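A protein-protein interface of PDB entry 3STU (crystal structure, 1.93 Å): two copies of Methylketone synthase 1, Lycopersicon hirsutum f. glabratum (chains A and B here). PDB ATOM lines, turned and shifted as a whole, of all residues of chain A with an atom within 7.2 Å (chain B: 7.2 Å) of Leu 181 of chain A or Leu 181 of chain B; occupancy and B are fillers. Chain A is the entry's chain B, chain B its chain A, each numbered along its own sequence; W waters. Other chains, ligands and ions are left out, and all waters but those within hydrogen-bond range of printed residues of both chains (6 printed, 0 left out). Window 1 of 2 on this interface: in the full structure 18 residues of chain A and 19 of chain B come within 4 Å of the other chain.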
ATOM      1  N   PHE A  22     -20.384 -24.907  -2.028  1.00  0.00           N
ATOM      2  CA  PHE A  22     -21.111 -25.781  -2.966  1.00  0.00           C
ATOM      3  C   PHE A  22     -22.454 -25.210  -3.412  1.00  0.00           C
ATOM      4  O   PHE A  22     -23.029 -25.672  -4.398  1.00  0.00           O
ATOM      5  CB  PHE A  22     -21.323 -27.208  -2.403  1.00  0.00           C
ATOM      6  CG  PHE A  22     -20.133 -27.759  -1.651  1.00  0.00           C
ATOM      7  CD1 PHE A  22     -18.916 -27.961  -2.293  1.00  0.00           C
ATOM      8  CD2 PHE A  22     -20.242 -28.085  -0.299  1.00  0.00           C
ATOM      9  CE1 PHE A  22     -17.819 -28.470  -1.592  1.00  0.00           C
ATOM     10  CE2 PHE A  22     -19.158 -28.588   0.409  1.00  0.00           C
ATOM     11  CZ  PHE A  22     -17.941 -28.784  -0.242  1.00  0.00           C
ATOM     12  N   HIS A  23     -22.952 -24.213  -2.685  1.00  0.00           N
ATOM     13  CA  HIS A  23     -24.304 -23.711  -2.894  1.00  0.00           C
ATOM     14  C   HIS A  23     -24.330 -22.459  -3.774  1.00  0.00           C
ATOM     15  O   HIS A  23     -23.333 -22.116  -4.395  1.00  0.00           O
ATOM     16  CB  HIS A  23     -24.988 -23.488  -1.539  1.00  0.00           C
ATOM     17  CG  HIS A  23     -25.420 -24.762  -0.880  1.00  0.00           C
ATOM     18  ND1 HIS A  23     -24.524 -25.717  -0.444  1.00  0.00           N
ATOM     19  CD2 HIS A  23     -26.653 -25.253  -0.613  1.00  0.00           C
ATOM     20  CE1 HIS A  23     -25.186 -26.737   0.072  1.00  0.00           C
ATOM     21  NE2 HIS A  23     -26.480 -26.481  -0.019  1.00  0.00           N
ATOM     22  N   GLY A  24     -25.477 -21.796  -3.848  1.00  0.00           N
ATOM     23  CA  GLY A  24     -25.607 -20.566  -4.630  1.00  0.00           C
ATOM     24  C   GLY A  24     -26.757 -19.744  -4.103  1.00  0.00           C
ATOM     25  O   GLY A  24     -27.316 -20.073  -3.057  1.00  0.00           O
ATOM     26  N   ALA A  25     -27.099 -18.671  -4.815  1.00  0.00           N
ATOM     27  CA  ALA A  25     -28.244 -17.836  -4.472  1.00  0.00           C
ATOM     28  C   ALA A  25     -29.525 -18.662  -4.333  1.00  0.00           C
ATOM     29  O   ALA A  25     -30.394 -18.339  -3.526  1.00  0.00           O
ATOM     30  CB  ALA A  25     -28.433 -16.748  -5.509  1.00  0.00           C
ATOM     31  N   TRP A  26     -29.615 -19.737  -5.118  1.00  0.00           N
ATOM     32  CA  TRP A  26     -30.801 -20.585  -5.161  1.00  0.00           C
ATOM     33  C   TRP A  26     -31.211 -21.161  -3.806  1.00  0.00           C
ATOM     34  O   TRP A  26     -32.401 -21.378  -3.570  1.00  0.00           O
ATOM     35  CB  TRP A  26     -30.603 -21.729  -6.149  1.00  0.00           C
ATOM     36  CG  TRP A  26     -29.396 -22.581  -5.863  1.00  0.00           C
ATOM     37  CD1 TRP A  26     -28.140 -22.422  -6.383  1.00  0.00           C
ATOM     38  CD2 TRP A  26     -29.330 -23.732  -5.005  1.00  0.00           C
ATOM     39  NE1 TRP A  26     -27.301 -23.398  -5.902  1.00  0.00           N
ATOM     40  CE2 TRP A  26     -28.003 -24.216  -5.058  1.00  0.00           C
ATOM     41  CE3 TRP A  26     -30.265 -24.407  -4.208  1.00  0.00           C
ATOM     42  CZ2 TRP A  26     -27.581 -25.333  -4.330  1.00  0.00           C
ATOM     43  CZ3 TRP A  26     -29.843 -25.522  -3.485  1.00  0.00           C
ATOM     44  CH2 TRP A  26     -28.512 -25.971  -3.553  1.00  0.00           C
ATOM     45  N   CYS A  27     -30.244 -21.406  -2.919  1.00  0.00           N
ATOM     46  CA  CYS A  27     -30.552 -22.077  -1.642  1.00  0.00           C
ATOM     47  C   CYS A  27     -31.436 -21.223  -0.737  1.00  0.00           C
ATOM     48  O   CYS A  27     -32.109 -21.751   0.156  1.00  0.00           O
ATOM     49  CB  CYS A  27     -29.275 -22.526  -0.907  1.00  0.00           C
ATOM     50  SG  CYS A  27     -28.373 -21.189  -0.113  1.00  0.00           S
ATOM     51  N   ASP A  46     -24.747 -15.040  -6.010  1.00  0.00           N
ATOM     52  CA  ASP A  46     -23.861 -16.159  -6.320  1.00  0.00           C
ATOM     53  C   ASP A  46     -22.423 -15.671  -6.141  1.00  0.00           C
ATOM     54  O   ASP A  46     -22.019 -14.670  -6.753  1.00  0.00           O
ATOM     55  CB  ASP A  46     -24.030 -16.624  -7.775  1.00  0.00           C
ATOM     56  CG  ASP A  46     -25.291 -17.449  -8.009  1.00  0.00           C
ATOM     57  OD1 ASP A  46     -25.733 -18.185  -7.097  1.00  0.00           O
ATOM     58  OD2 ASP A  46     -25.830 -17.374  -9.137  1.00  0.00           O
ATOM     59  N   SER A  50     -20.336 -20.409  -8.261  1.00  0.00           N
ATOM     60  CA  SER A  50     -21.428 -20.916  -7.444  1.00  0.00           C
ATOM     61  C   SER A  50     -22.725 -20.623  -8.175  1.00  0.00           C
ATOM     62  O   SER A  50     -22.823 -19.622  -8.888  1.00  0.00           O
ATOM     63  CB  SER A  50     -21.435 -20.203  -6.095  1.00  0.00           C
ATOM     64  OG  SER A  50     -20.173 -20.302  -5.458  1.00  0.00           O
ATOM     65  N   GLY A  51     -23.718 -21.498  -8.020  1.00  0.00           N
ATOM     66  CA  GLY A  51     -25.009 -21.314  -8.701  1.00  0.00           C
ATOM     67  C   GLY A  51     -24.828 -21.136 -10.198  1.00  0.00           C
ATOM     68  O   GLY A  51     -24.216 -21.985 -10.855  1.00  0.00           O
ATOM     69  N   ILE A  52     -25.321 -20.019 -10.734  1.00  0.00           N
ATOM     70  CA  ILE A  52     -25.179 -19.739 -12.166  1.00  0.00           C
ATOM     71  C   ILE A  52     -24.098 -18.698 -12.511  1.00  0.00           C
ATOM     72  O   ILE A  52     -24.079 -18.149 -13.621  1.00  0.00           O
ATOM     73  CB  ILE A  52     -26.545 -19.440 -12.870  1.00  0.00           C
ATOM     74  CG1 ILE A  52     -27.198 -18.162 -12.331  1.00  0.00           C
ATOM     75  CG2 ILE A  52     -27.489 -20.651 -12.755  1.00  0.00           C
ATOM     76  CD1 ILE A  52     -28.208 -17.531 -13.301  1.00  0.00           C
ATOM     77  N   LEU A 175     -33.351 -31.764  -0.799  1.00  0.00           N
ATOM     78  CA  LEU A 175     -32.169 -32.586  -1.053  1.00  0.00           C
ATOM     79  C   LEU A 175     -32.028 -32.853  -2.555  1.00  0.00           C
ATOM     80  O   LEU A 175     -30.946 -32.698  -3.117  1.00  0.00           O
ATOM     81  CB  LEU A 175     -32.236 -33.904  -0.279  1.00  0.00           C
ATOM     82  CG  LEU A 175     -31.177 -34.949  -0.654  1.00  0.00           C
ATOM     83  CD1 LEU A 175     -29.775 -34.482  -0.238  1.00  0.00           C
ATOM     84  CD2 LEU A 175     -31.505 -36.309  -0.048  1.00  0.00           C
ATOM     85  N   ALA A 176     -33.129 -33.242  -3.200  1.00  0.00           N
ATOM     86  CA  ALA A 176     -33.141 -33.443  -4.652  1.00  0.00           C
ATOM     87  C   ALA A 176     -32.703 -32.181  -5.400  1.00  0.00           C
ATOM     88  O   ALA A 176     -31.895 -32.254  -6.337  1.00  0.00           O
ATOM     89  CB  ALA A 176     -34.513 -33.902  -5.122  1.00  0.00           C
ATOM     90  N   LEU A 177     -33.217 -31.028  -4.977  1.00  0.00           N
ATOM     91  CA  LEU A 177     -32.824 -29.751  -5.586  1.00  0.00           C
ATOM     92  C   LEU A 177     -31.313 -29.524  -5.456  1.00  0.00           C
ATOM     93  O   LEU A 177     -30.633 -29.224  -6.446  1.00  0.00           O
ATOM     94  CB  LEU A 177     -33.617 -28.593  -4.968  1.00  0.00           C
ATOM     95  CG  LEU A 177     -33.386 -27.156  -5.470  1.00  0.00           C
ATOM     96  CD1 LEU A 177     -33.770 -26.991  -6.934  1.00  0.00           C
ATOM     97  CD2 LEU A 177     -34.182 -26.172  -4.610  1.00  0.00           C
ATOM     98  N   ALA A 178     -30.793 -29.704  -4.242  1.00  0.00           N
ATOM     99  CA  ALA A 178     -29.365 -29.548  -3.963  1.00  0.00           C
ATOM    100  C   ALA A 178     -28.477 -30.447  -4.825  1.00  0.00           C
ATOM    101  O   ALA A 178     -27.458 -29.998  -5.357  1.00  0.00           O
ATOM    102  CB  ALA A 178     -29.083 -29.792  -2.478  1.00  0.00           C
ATOM    103  N   THR A 179     -28.866 -31.709  -4.977  1.00  0.00           N
ATOM    104  CA  THR A 179     -28.035 -32.647  -5.729  1.00  0.00           C
ATOM    105  C   THR A 179     -27.956 -32.281  -7.216  1.00  0.00           C
ATOM    106  O   THR A 179     -26.946 -32.544  -7.867  1.00  0.00           O
ATOM    107  CB  THR A 179     -28.445 -34.136  -5.502  1.00  0.00           C
ATOM    108  OG1 THR A 179     -29.752 -34.367  -6.009  1.00  0.00           O
ATOM    109  CG2 THR A 179     -28.443 -34.470  -4.027  1.00  0.00           C
ATOM    110  N   ALA A 180     -29.003 -31.644  -7.739  1.00  0.00           N
ATOM    111  CA  ALA A 180     -28.968 -31.119  -9.101  1.00  0.00           C
ATOM    112  C   ALA A 180     -28.245 -29.767  -9.247  1.00  0.00           C
ATOM    113  O   ALA A 180     -28.049 -29.310 -10.373  1.00  0.00           O
ATOM    114  CB  ALA A 180     -30.389 -31.020  -9.675  1.00  0.00           C
ATOM    115  N   LEU A 181     -27.862 -29.134  -8.133  1.00  0.00           N
ATOM    116  CA  LEU A 181     -27.303 -27.766  -8.191  1.00  0.00           C
ATOM    117  C   LEU A 181     -25.932 -27.518  -7.550  1.00  0.00           C
ATOM    118  O   LEU A 181     -25.252 -26.536  -7.887  1.00  0.00           O
ATOM    119  CB  LEU A 181     -28.302 -26.739  -7.638  1.00  0.00           C
ATOM    120  CG  LEU A 181     -29.534 -26.450  -8.498  1.00  0.00           C
ATOM    121  CD1 LEU A 181     -30.587 -25.690  -7.705  1.00  0.00           C
ATOM    122  CD2 LEU A 181     -29.172 -25.713  -9.790  1.00  0.00           C
ATOM    123  N   VAL A 182     -25.533 -28.360  -6.602  1.00  0.00           N
ATOM    124  CA  VAL A 182     -24.254 -28.143  -5.925  1.00  0.00           C
ATOM    125  C   VAL A 182     -23.091 -28.208  -6.913  1.00  0.00           C
ATOM    126  O   VAL A 182     -23.081 -29.039  -7.823  1.00  0.00           O
ATOM    127  CB  VAL A 182     -24.020 -29.101  -4.727  1.00  0.00           C
ATOM    128  CG1 VAL A 182     -24.975 -28.748  -3.581  1.00  0.00           C
ATOM    129  CG2 VAL A 182     -24.161 -30.566  -5.157  1.00  0.00           C
ATOM    130  N   ARG A 183     -22.138 -27.298  -6.742  1.00  0.00           N
ATOM    131  CA  ARG A 183     -20.971 -27.217  -7.619  1.00  0.00           C
ATOM    132  C   ARG A 183     -19.695 -27.387  -6.793  1.00  0.00           C
ATOM    133  O   ARG A 183     -19.729 -27.184  -5.583  1.00  0.00           O
ATOM    134  CB  ARG A 183     -20.965 -25.878  -8.359  1.00  0.00           C
ATOM    135  CG  ARG A 183     -22.151 -25.712  -9.315  1.00  0.00           C
ATOM    136  CD  ARG A 183     -22.120 -24.356 -10.006  1.00  0.00           C
ATOM    137  NE  ARG A 183     -20.951 -24.214 -10.878  1.00  0.00           N
ATOM    138  CZ  ARG A 183     -20.586 -23.076 -11.462  1.00  0.00           C
ATOM    139  NH1 ARG A 183     -21.286 -21.966 -11.274  1.00  0.00           N
ATOM    140  NH2 ARG A 183     -19.506 -23.048 -12.233  1.00  0.00           N
ATOM    141  N   PRO A 184     -18.573 -27.773  -7.441  1.00  0.00           N
ATOM    142  CA  PRO A 184     -17.299 -27.937  -6.727  1.00  0.00           C
ATOM    143  C   PRO A 184     -16.821 -26.640  -6.090  1.00  0.00           C
ATOM    144  O   PRO A 184     -17.170 -25.557  -6.566  1.00  0.00           O
ATOM    145  CB  PRO A 184     -16.319 -28.351  -7.835  1.00  0.00           C
ATOM    146  CG  PRO A 184     -17.175 -28.907  -8.919  1.00  0.00           C
ATOM    147  CD  PRO A 184     -18.459 -28.148  -8.863  1.00  0.00           C
ATOM    148  N   PHE B  22     -34.499 -21.872 -20.802  1.00  0.00           N
ATOM    149  CA  PHE B  22     -34.109 -21.108 -19.605  1.00  0.00           C
ATOM    150  C   PHE B  22     -33.938 -21.962 -18.357  1.00  0.00           C
ATOM    151  O   PHE B  22     -33.322 -21.521 -17.387  1.00  0.00           O
ATOM    152  CB  PHE B  22     -35.086 -19.960 -19.285  1.00  0.00           C
ATOM    153  CG  PHE B  22     -35.586 -19.219 -20.489  1.00  0.00           C
ATOM    154  CD1 PHE B  22     -34.698 -18.612 -21.374  1.00  0.00           C
ATOM    155  CD2 PHE B  22     -36.959 -19.115 -20.728  1.00  0.00           C
ATOM    156  CE1 PHE B  22     -35.164 -17.916 -22.481  1.00  0.00           C
ATOM    157  CE2 PHE B  22     -37.442 -18.424 -21.838  1.00  0.00           C
ATOM    158  CZ  PHE B  22     -36.540 -17.829 -22.721  1.00  0.00           C
ATOM    159  N   HIS B  23     -34.495 -23.168 -18.374  1.00  0.00           N
ATOM    160  CA  HIS B  23     -34.537 -23.997 -17.182  1.00  0.00           C
ATOM    161  C   HIS B  23     -33.391 -24.999 -17.137  1.00  0.00           C
ATOM    162  O   HIS B  23     -32.470 -24.914 -17.931  1.00  0.00           O
ATOM    163  CB  HIS B  23     -35.913 -24.665 -17.050  1.00  0.00           C
ATOM    164  CG  HIS B  23     -36.987 -23.703 -16.649  1.00  0.00           C
ATOM    165  ND1 HIS B  23     -37.466 -22.731 -17.500  1.00  0.00           N
ATOM    166  CD2 HIS B  23     -37.628 -23.519 -15.470  1.00  0.00           C
ATOM    167  CE1 HIS B  23     -38.382 -22.013 -16.874  1.00  0.00           C
ATOM    168  NE2 HIS B  23     -38.500 -22.472 -15.641  1.00  0.00           N
ATOM    169  N   GLY B  24     -33.449 -25.927 -16.190  1.00  0.00           N
ATOM    170  CA  GLY B  24     -32.401 -26.917 -16.015  1.00  0.00           C
ATOM    171  C   GLY B  24     -32.960 -28.116 -15.277  1.00  0.00           C
ATOM    172  O   GLY B  24     -34.160 -28.173 -14.990  1.00  0.00           O
ATOM    173  N   ALA B  25     -32.089 -29.058 -14.951  1.00  0.00           N
ATOM    174  CA  ALA B  25     -32.465 -30.238 -14.163  1.00  0.00           C
ATOM    175  C   ALA B  25     -33.184 -29.854 -12.871  1.00  0.00           C
ATOM    176  O   ALA B  25     -34.091 -30.564 -12.422  1.00  0.00           O
ATOM    177  CB  ALA B  25     -31.232 -31.063 -13.845  1.00  0.00           C
ATOM    178  N   TRP B  26     -32.784 -28.719 -12.294  1.00  0.00           N
ATOM    179  CA  TRP B  26     -33.336 -28.243 -11.028  1.00  0.00           C
ATOM    180  C   TRP B  26     -34.857 -28.096 -11.025  1.00  0.00           C
ATOM    181  O   TRP B  26     -35.493 -28.246  -9.984  1.00  0.00           O
ATOM    182  CB  TRP B  26     -32.703 -26.909 -10.640  1.00  0.00           C
ATOM    183  CG  TRP B  26     -32.879 -25.825 -11.674  1.00  0.00           C
ATOM    184  CD1 TRP B  26     -32.004 -25.507 -12.680  1.00  0.00           C
ATOM    185  CD2 TRP B  26     -33.989 -24.917 -11.807  1.00  0.00           C
ATOM    186  NE1 TRP B  26     -32.496 -24.454 -13.417  1.00  0.00           N
ATOM    187  CE2 TRP B  26     -33.708 -24.071 -12.902  1.00  0.00           C
ATOM    188  CE3 TRP B  26     -35.182 -24.719 -11.090  1.00  0.00           C
ATOM    189  CZ2 TRP B  26     -34.593 -23.057 -13.322  1.00  0.00           C
ATOM    190  CZ3 TRP B  26     -36.057 -23.704 -11.507  1.00  0.00           C
ATOM    191  CH2 TRP B  26     -35.752 -22.889 -12.612  1.00  0.00           C
ATOM    192  N   CYS B  27     -35.445 -27.804 -12.181  1.00  0.00           N
ATOM    193  CA  CYS B  27     -36.873 -27.507 -12.214  1.00  0.00           C
ATOM    194  C   CYS B  27     -37.731 -28.739 -11.919  1.00  0.00           C
ATOM    195  O   CYS B  27     -38.874 -28.606 -11.500  1.00  0.00           O
ATOM    196  CB  CYS B  27     -37.284 -26.842 -13.534  1.00  0.00           C
ATOM    197  SG  CYS B  27     -37.469 -27.977 -14.922  1.00  0.00           S
ATOM    198  N   ASP B  46     -29.222 -31.462 -17.372  1.00  0.00           N
ATOM    199  CA  ASP B  46     -29.014 -30.102 -17.861  1.00  0.00           C
ATOM    200  C   ASP B  46     -28.614 -30.195 -19.329  1.00  0.00           C
ATOM    201  O   ASP B  46     -27.619 -30.853 -19.662  1.00  0.00           O
ATOM    202  CB  ASP B  46     -27.885 -29.404 -17.097  1.00  0.00           C
ATOM    203  CG  ASP B  46     -28.273 -29.001 -15.685  1.00  0.00           C
ATOM    204  OD1 ASP B  46     -29.456 -28.704 -15.433  1.00  0.00           O
ATOM    205  OD2 ASP B  46     -27.371 -28.943 -14.823  1.00  0.00           O
ATOM    206  N   SER B  50     -27.428 -24.734 -19.499  1.00  0.00           N
ATOM    207  CA  SER B  50     -28.635 -24.749 -18.672  1.00  0.00           C
ATOM    208  C   SER B  50     -28.278 -25.287 -17.283  1.00  0.00           C
ATOM    209  O   SER B  50     -27.398 -26.137 -17.153  1.00  0.00           O
ATOM    210  CB  SER B  50     -29.698 -25.650 -19.300  1.00  0.00           C
ATOM    211  OG  SER B  50     -29.854 -25.413 -20.692  1.00  0.00           O
ATOM    212  N   GLY B  51     -28.955 -24.792 -16.247  1.00  0.00           N
ATOM    213  CA  GLY B  51     -28.662 -25.206 -14.883  1.00  0.00           C
ATOM    214  C   GLY B  51     -27.185 -25.002 -14.575  1.00  0.00           C
ATOM    215  O   GLY B  51     -26.665 -23.897 -14.715  1.00  0.00           O
ATOM    216  N   ILE B  52     -26.507 -26.078 -14.185  1.00  0.00           N
ATOM    217  CA  ILE B  52     -25.081 -26.009 -13.864  1.00  0.00           C
ATOM    218  C   ILE B  52     -24.187 -26.609 -14.961  1.00  0.00           C
ATOM    219  O   ILE B  52     -23.015 -26.909 -14.726  1.00  0.00           O
ATOM    220  CB  ILE B  52     -24.750 -26.626 -12.463  1.00  0.00           C
ATOM    221  CG1 ILE B  52     -25.182 -28.096 -12.395  1.00  0.00           C
ATOM    222  CG2 ILE B  52     -25.395 -25.782 -11.340  1.00  0.00           C
ATOM    223  CD1 ILE B  52     -24.561 -28.883 -11.255  1.00  0.00           C
ATOM    224  N   LEU B 175     -41.197 -19.418  -8.008  1.00  0.00           N
ATOM    225  CA  LEU B 175     -40.866 -18.237  -8.785  1.00  0.00           C
ATOM    226  C   LEU B 175     -39.524 -17.658  -8.335  1.00  0.00           C
ATOM    227  O   LEU B 175     -38.688 -17.341  -9.177  1.00  0.00           O
ATOM    228  CB  LEU B 175     -41.982 -17.179  -8.722  1.00  0.00           C
ATOM    229  CG  LEU B 175     -41.683 -15.803  -9.338  1.00  0.00           C
ATOM    230  CD1 LEU B 175     -41.364 -15.886 -10.840  1.00  0.00           C
ATOM    231  CD2 LEU B 175     -42.861 -14.888  -9.085  1.00  0.00           C
ATOM    232  N   ALA B 176     -39.311 -17.534  -7.022  1.00  0.00           N
ATOM    233  CA  ALA B 176     -38.041 -17.001  -6.516  1.00  0.00           C
ATOM    234  C   ALA B 176     -36.874 -17.894  -6.918  1.00  0.00           C
ATOM    235  O   ALA B 176     -35.822 -17.395  -7.316  1.00  0.00           O
ATOM    236  CB  ALA B 176     -38.072 -16.808  -4.998  1.00  0.00           C
ATOM    237  N   LEU B 177     -37.080 -19.209  -6.826  1.00  0.00           N
ATOM    238  CA  LEU B 177     -36.083 -20.202  -7.238  1.00  0.00           C
ATOM    239  C   LEU B 177     -35.694 -20.022  -8.704  1.00  0.00           C
ATOM    240  O   LEU B 177     -34.504 -19.982  -9.048  1.00  0.00           O
ATOM    241  CB  LEU B 177     -36.614 -21.626  -6.990  1.00  0.00           C
ATOM    242  CG  LEU B 177     -35.681 -22.811  -7.291  1.00  0.00           C
ATOM    243  CD1 LEU B 177     -34.412 -22.760  -6.428  1.00  0.00           C
ATOM    244  CD2 LEU B 177     -36.405 -24.150  -7.094  1.00  0.00           C
ATOM    245  N   ALA B 178     -36.709 -19.887  -9.557  1.00  0.00           N
ATOM    246  CA  ALA B 178     -36.508 -19.689 -10.984  1.00  0.00           C
ATOM    247  C   ALA B 178     -35.757 -18.404 -11.284  1.00  0.00           C
ATOM    248  O   ALA B 178     -34.857 -18.390 -12.125  1.00  0.00           O
ATOM    249  CB  ALA B 178     -37.837 -19.693 -11.713  1.00  0.00           C
ATOM    250  N   THR B 179     -36.126 -17.326 -10.595  1.00  0.00           N
ATOM    251  CA  THR B 179     -35.475 -16.043 -10.820  1.00  0.00           C
ATOM    252  C   THR B 179     -33.981 -16.112 -10.516  1.00  0.00           C
ATOM    253  O   THR B 179     -33.203 -15.392 -11.135  1.00  0.00           O
ATOM    254  CB  THR B 179     -36.153 -14.887 -10.053  1.00  0.00           C
ATOM    255  OG1 THR B 179     -36.136 -15.165  -8.648  1.00  0.00           O
ATOM    256  CG2 THR B 179     -37.593 -14.707 -10.520  1.00  0.00           C
ATOM    257  N   ALA B 180     -33.580 -16.998  -9.599  1.00  0.00           N
ATOM    258  CA  ALA B 180     -32.166 -17.145  -9.238  1.00  0.00           C
ATOM    259  C   ALA B 180     -31.409 -18.105 -10.156  1.00  0.00           C
ATOM    260  O   ALA B 180     -30.183 -18.164 -10.097  1.00  0.00           O
ATOM    261  CB  ALA B 180     -32.025 -17.581  -7.773  1.00  0.00           C
ATOM    262  N   LEU B 181     -32.139 -18.848 -10.996  1.00  0.00           N
ATOM    263  CA  LEU B 181     -31.559 -19.962 -11.767  1.00  0.00           C
ATOM    264  C   LEU B 181     -31.722 -19.942 -13.292  1.00  0.00           C
ATOM    265  O   LEU B 181     -30.963 -20.624 -13.999  1.00  0.00           O
ATOM    266  CB  LEU B 181     -32.090 -21.299 -11.232  1.00  0.00           C
ATOM    267  CG  LEU B 181     -31.578 -21.719  -9.856  1.00  0.00           C
ATOM    268  CD1 LEU B 181     -32.321 -22.981  -9.401  1.00  0.00           C
ATOM    269  CD2 LEU B 181     -30.052 -21.954  -9.861  1.00  0.00           C
ATOM    270  N   VAL B 182     -32.699 -19.189 -13.809  1.00  0.00           N
ATOM    271  CA  VAL B 182     -32.907 -19.143 -15.271  1.00  0.00           C
ATOM    272  C   VAL B 182     -31.675 -18.563 -15.959  1.00  0.00           C
ATOM    273  O   VAL B 182     -31.038 -17.634 -15.447  1.00  0.00           O
ATOM    274  CB  VAL B 182     -34.193 -18.362 -15.712  1.00  0.00           C
ATOM    275  CG1 VAL B 182     -35.472 -19.154 -15.366  1.00  0.00           C
ATOM    276  CG2 VAL B 182     -34.218 -16.938 -15.129  1.00  0.00           C
ATOM    277  N   ARG B 183     -31.330 -19.146 -17.101  1.00  0.00           N
ATOM    278  CA  ARG B 183     -30.155 -18.743 -17.867  1.00  0.00           C
ATOM    279  C   ARG B 183     -30.582 -18.400 -19.295  1.00  0.00           C
ATOM    280  O   ARG B 183     -31.657 -18.817 -19.724  1.00  0.00           O
ATOM    281  CB  ARG B 183     -29.127 -19.879 -17.860  1.00  0.00           C
ATOM    282  CG  ARG B 183     -28.605 -20.222 -16.464  1.00  0.00           C
ATOM    283  CD  ARG B 183     -27.539 -21.301 -16.516  1.00  0.00           C
ATOM    284  NE  ARG B 183     -26.370 -20.878 -17.293  1.00  0.00           N
ATOM    285  CZ  ARG B 183     -25.355 -21.679 -17.625  1.00  0.00           C
ATOM    286  NH1 ARG B 183     -25.339 -22.960 -17.252  1.00  0.00           N
ATOM    287  NH2 ARG B 183     -24.346 -21.194 -18.336  1.00  0.00           N
ATOM    288  N   PRO B 184     -29.756 -17.628 -20.033  1.00  0.00           N
ATOM    289  CA  PRO B 184     -30.124 -17.237 -21.396  1.00  0.00           C
ATOM    290  C   PRO B 184     -30.238 -18.428 -22.327  1.00  0.00           C
ATOM    291  O   PRO B 184     -29.557 -19.431 -22.117  1.00  0.00           O
ATOM    292  CB  PRO B 184     -28.947 -16.355 -21.846  1.00  0.00           C
ATOM    293  CG  PRO B 184     -28.307 -15.890 -20.597  1.00  0.00           C
ATOM    294  CD  PRO B 184     -28.502 -16.983 -19.594  1.00  0.00           C
HETATM  295  O   HOH W   1     -27.553 -30.731 -12.772  1.00  0.00           O
HETATM  296  O   HOH W   2     -20.228 -25.778 -14.277  1.00  0.00           O
HETATM  297  O   HOH W   3     -29.860 -28.000 -12.605  1.00  0.00           O
HETATM  298  O   HOH W   4     -24.264 -22.705 -13.523  1.00  0.00           O
HETATM  299  O   HOH W   5     -28.503 -16.315  -9.307  1.00  0.00           O
HETATM  300  O   HOH W   6     -28.261 -19.515  -7.863  1.00  0.00           O
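O of Phe 22 of chain B lies within hydrogen-bond range of N of Arg 183 of chain B.
The backbone NH (N) of Ile 52 of chain B lies within hydrogen-bond range of the side-chain carboxylate (OD2) of Asp 46 of chain B (3.1 Å).
NH1 of Arg 183 of chain B is in hydrogen-bond range of O of Gly 51 of chain B, 3.0 Å away.
The backbone carbonyl oxygen (O) of Phe 22 of chain A is in hydrogen-bond range of the backbone NH (N) of Arg 183 of chain A (3.0 Å).
The side-chain carboxylate (OD2) of Asp 46 of chain A is in hydrogen-bond range of the backbone NH (N) of Ile 52 of chain A.
O of Gly 51 of chain A lies within hydrogen-bond range of NH1 of Arg 183 of chain A (3.0 Å).
Water W5 lies within hydrogen-bond range of the backbone carbonyl oxygen (O) of Ala 180 of chain B (2.6 Å) and the side-chain carboxylate (OD2) of Asp 46 of chain A (2.9 Å).
Water W1 bridges OD2 of Asp 46 of chain B (2.7 Å) and O of Ala 180 of chain A (2.8 Å).
Water W4 lies within hydrogen-bond range of the backbone carbonyl oxygen of Gly 51 of chain A (2.8 Å) and the backbone carbonyl oxygen of Gly 51 of chain B (2.9 Å).
Water W3 lies within hydrogen-bond range of OD1 of Asp 46 of chain B (2.9 Å), N of Trp 26 of chain B (3.0 Å), O of Ala 180 of chain A (3.2 Å) and N of Ala 25 of chain B (3.4 Å).
Water W6 lies within hydrogen-bond range of OD1 of Asp 46 of chain A, N of Trp 26 of chain A, O of Ala 180 of chain B and N of Ala 25 of chain A.
Water W2 bridges O of Ile 52 of chain B and NH2 of Arg 183 of chain A.
Of chain B, only Trp 26, Ile 52 and Leu 181 come within 4 Å of Leu 181 of chain A.
Leu 181 of chain B touches just these residues of chain A: Trp 26 (3.8 Å), Ile 52 (3.7 Å) and Leu 181 (3.6 Å).
Of the printed residues of chain A, Ile 52 of chain B touches Ala 180 (3.6 Å), Leu 181 (3.5 Å), Val 182 (3.7 Å) and Arg 183 (3.8 Å).
Of the printed residues of chain A, Gly 51 of chain B touches Ile 52 (3.9 Å).
Of the printed residues of chain A, Val 182 of chain B touches Ile 52 (3.6 Å).
The nearest residue of chain A that does not touch Leu 181 of chain B is Leu 177 of chain A (4.9 Å).
Trp 26 of chain A touches Leu 177 of chain B, and with the chains exchanged Leu 177 of chain A touches Trp 26 of chain B.
Trp 26 of chain A touches Leu 181 of chain B, and with the chains exchanged Leu 181 of chain A touches Trp 26 of chain B.
Ile 52 of chain A touches Gly 51 of chain B, but with the chains exchanged Gly 51 of chain A does not touch Ile 52 of chain B (4.01 Å).
Leu 177 of chain B touches its own counterpart, Leu 177 of chain A.
Positions printed for both chains: 22, 23, 24, 25, 26, 27, 46, 50, 51, 52, 175, 176, 177, 178, 179, 180, 181, 182, 183 and 184.
Printed residues of chain B that touch a printed residue of chain A: Trp 26, Gly 51, Ile 52, Leu 177, Ala 180, Leu 181, Val 182 and Arg 183.
Along chain B the printed residues that touch a printed residue of chain A span positions 26 to 183.
Among the printed residues, no Asp or Glu carboxylate lies within 4 Å of a Lys or Arg side-chain nitrogen of the other chain.
Trp 26 of chain A touches Leu 181 of chain B (CB to CD2, 3.8 Å).
Ile 52 of chain A touches Ala 180 of chain B.
Leu 181 of chain B touches Ile 52 of chain A.
Arg 183 of chain B touches Ile 52 of chain A.
O of Trp 26 of chain B touches CD1 of Leu 177 of chain A, at 3.7 Å.
CD2 of Leu 177 of chain A touches CD1 of Leu 177 of chain B, 3.9 Å away.
Ala 180 of chain A touches Ile 52 of chain B (O to CD1, 3.6 Å).
Leu 181 of chain A touches Ile 52 of chain B.
Leu 181 of chain A touches Leu 181 of chain B (CD1 to CD1, 3.6 Å).
Arg 183 of chain A touches Ile 52 of chain B (CD to CG2, 3.8 Å).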
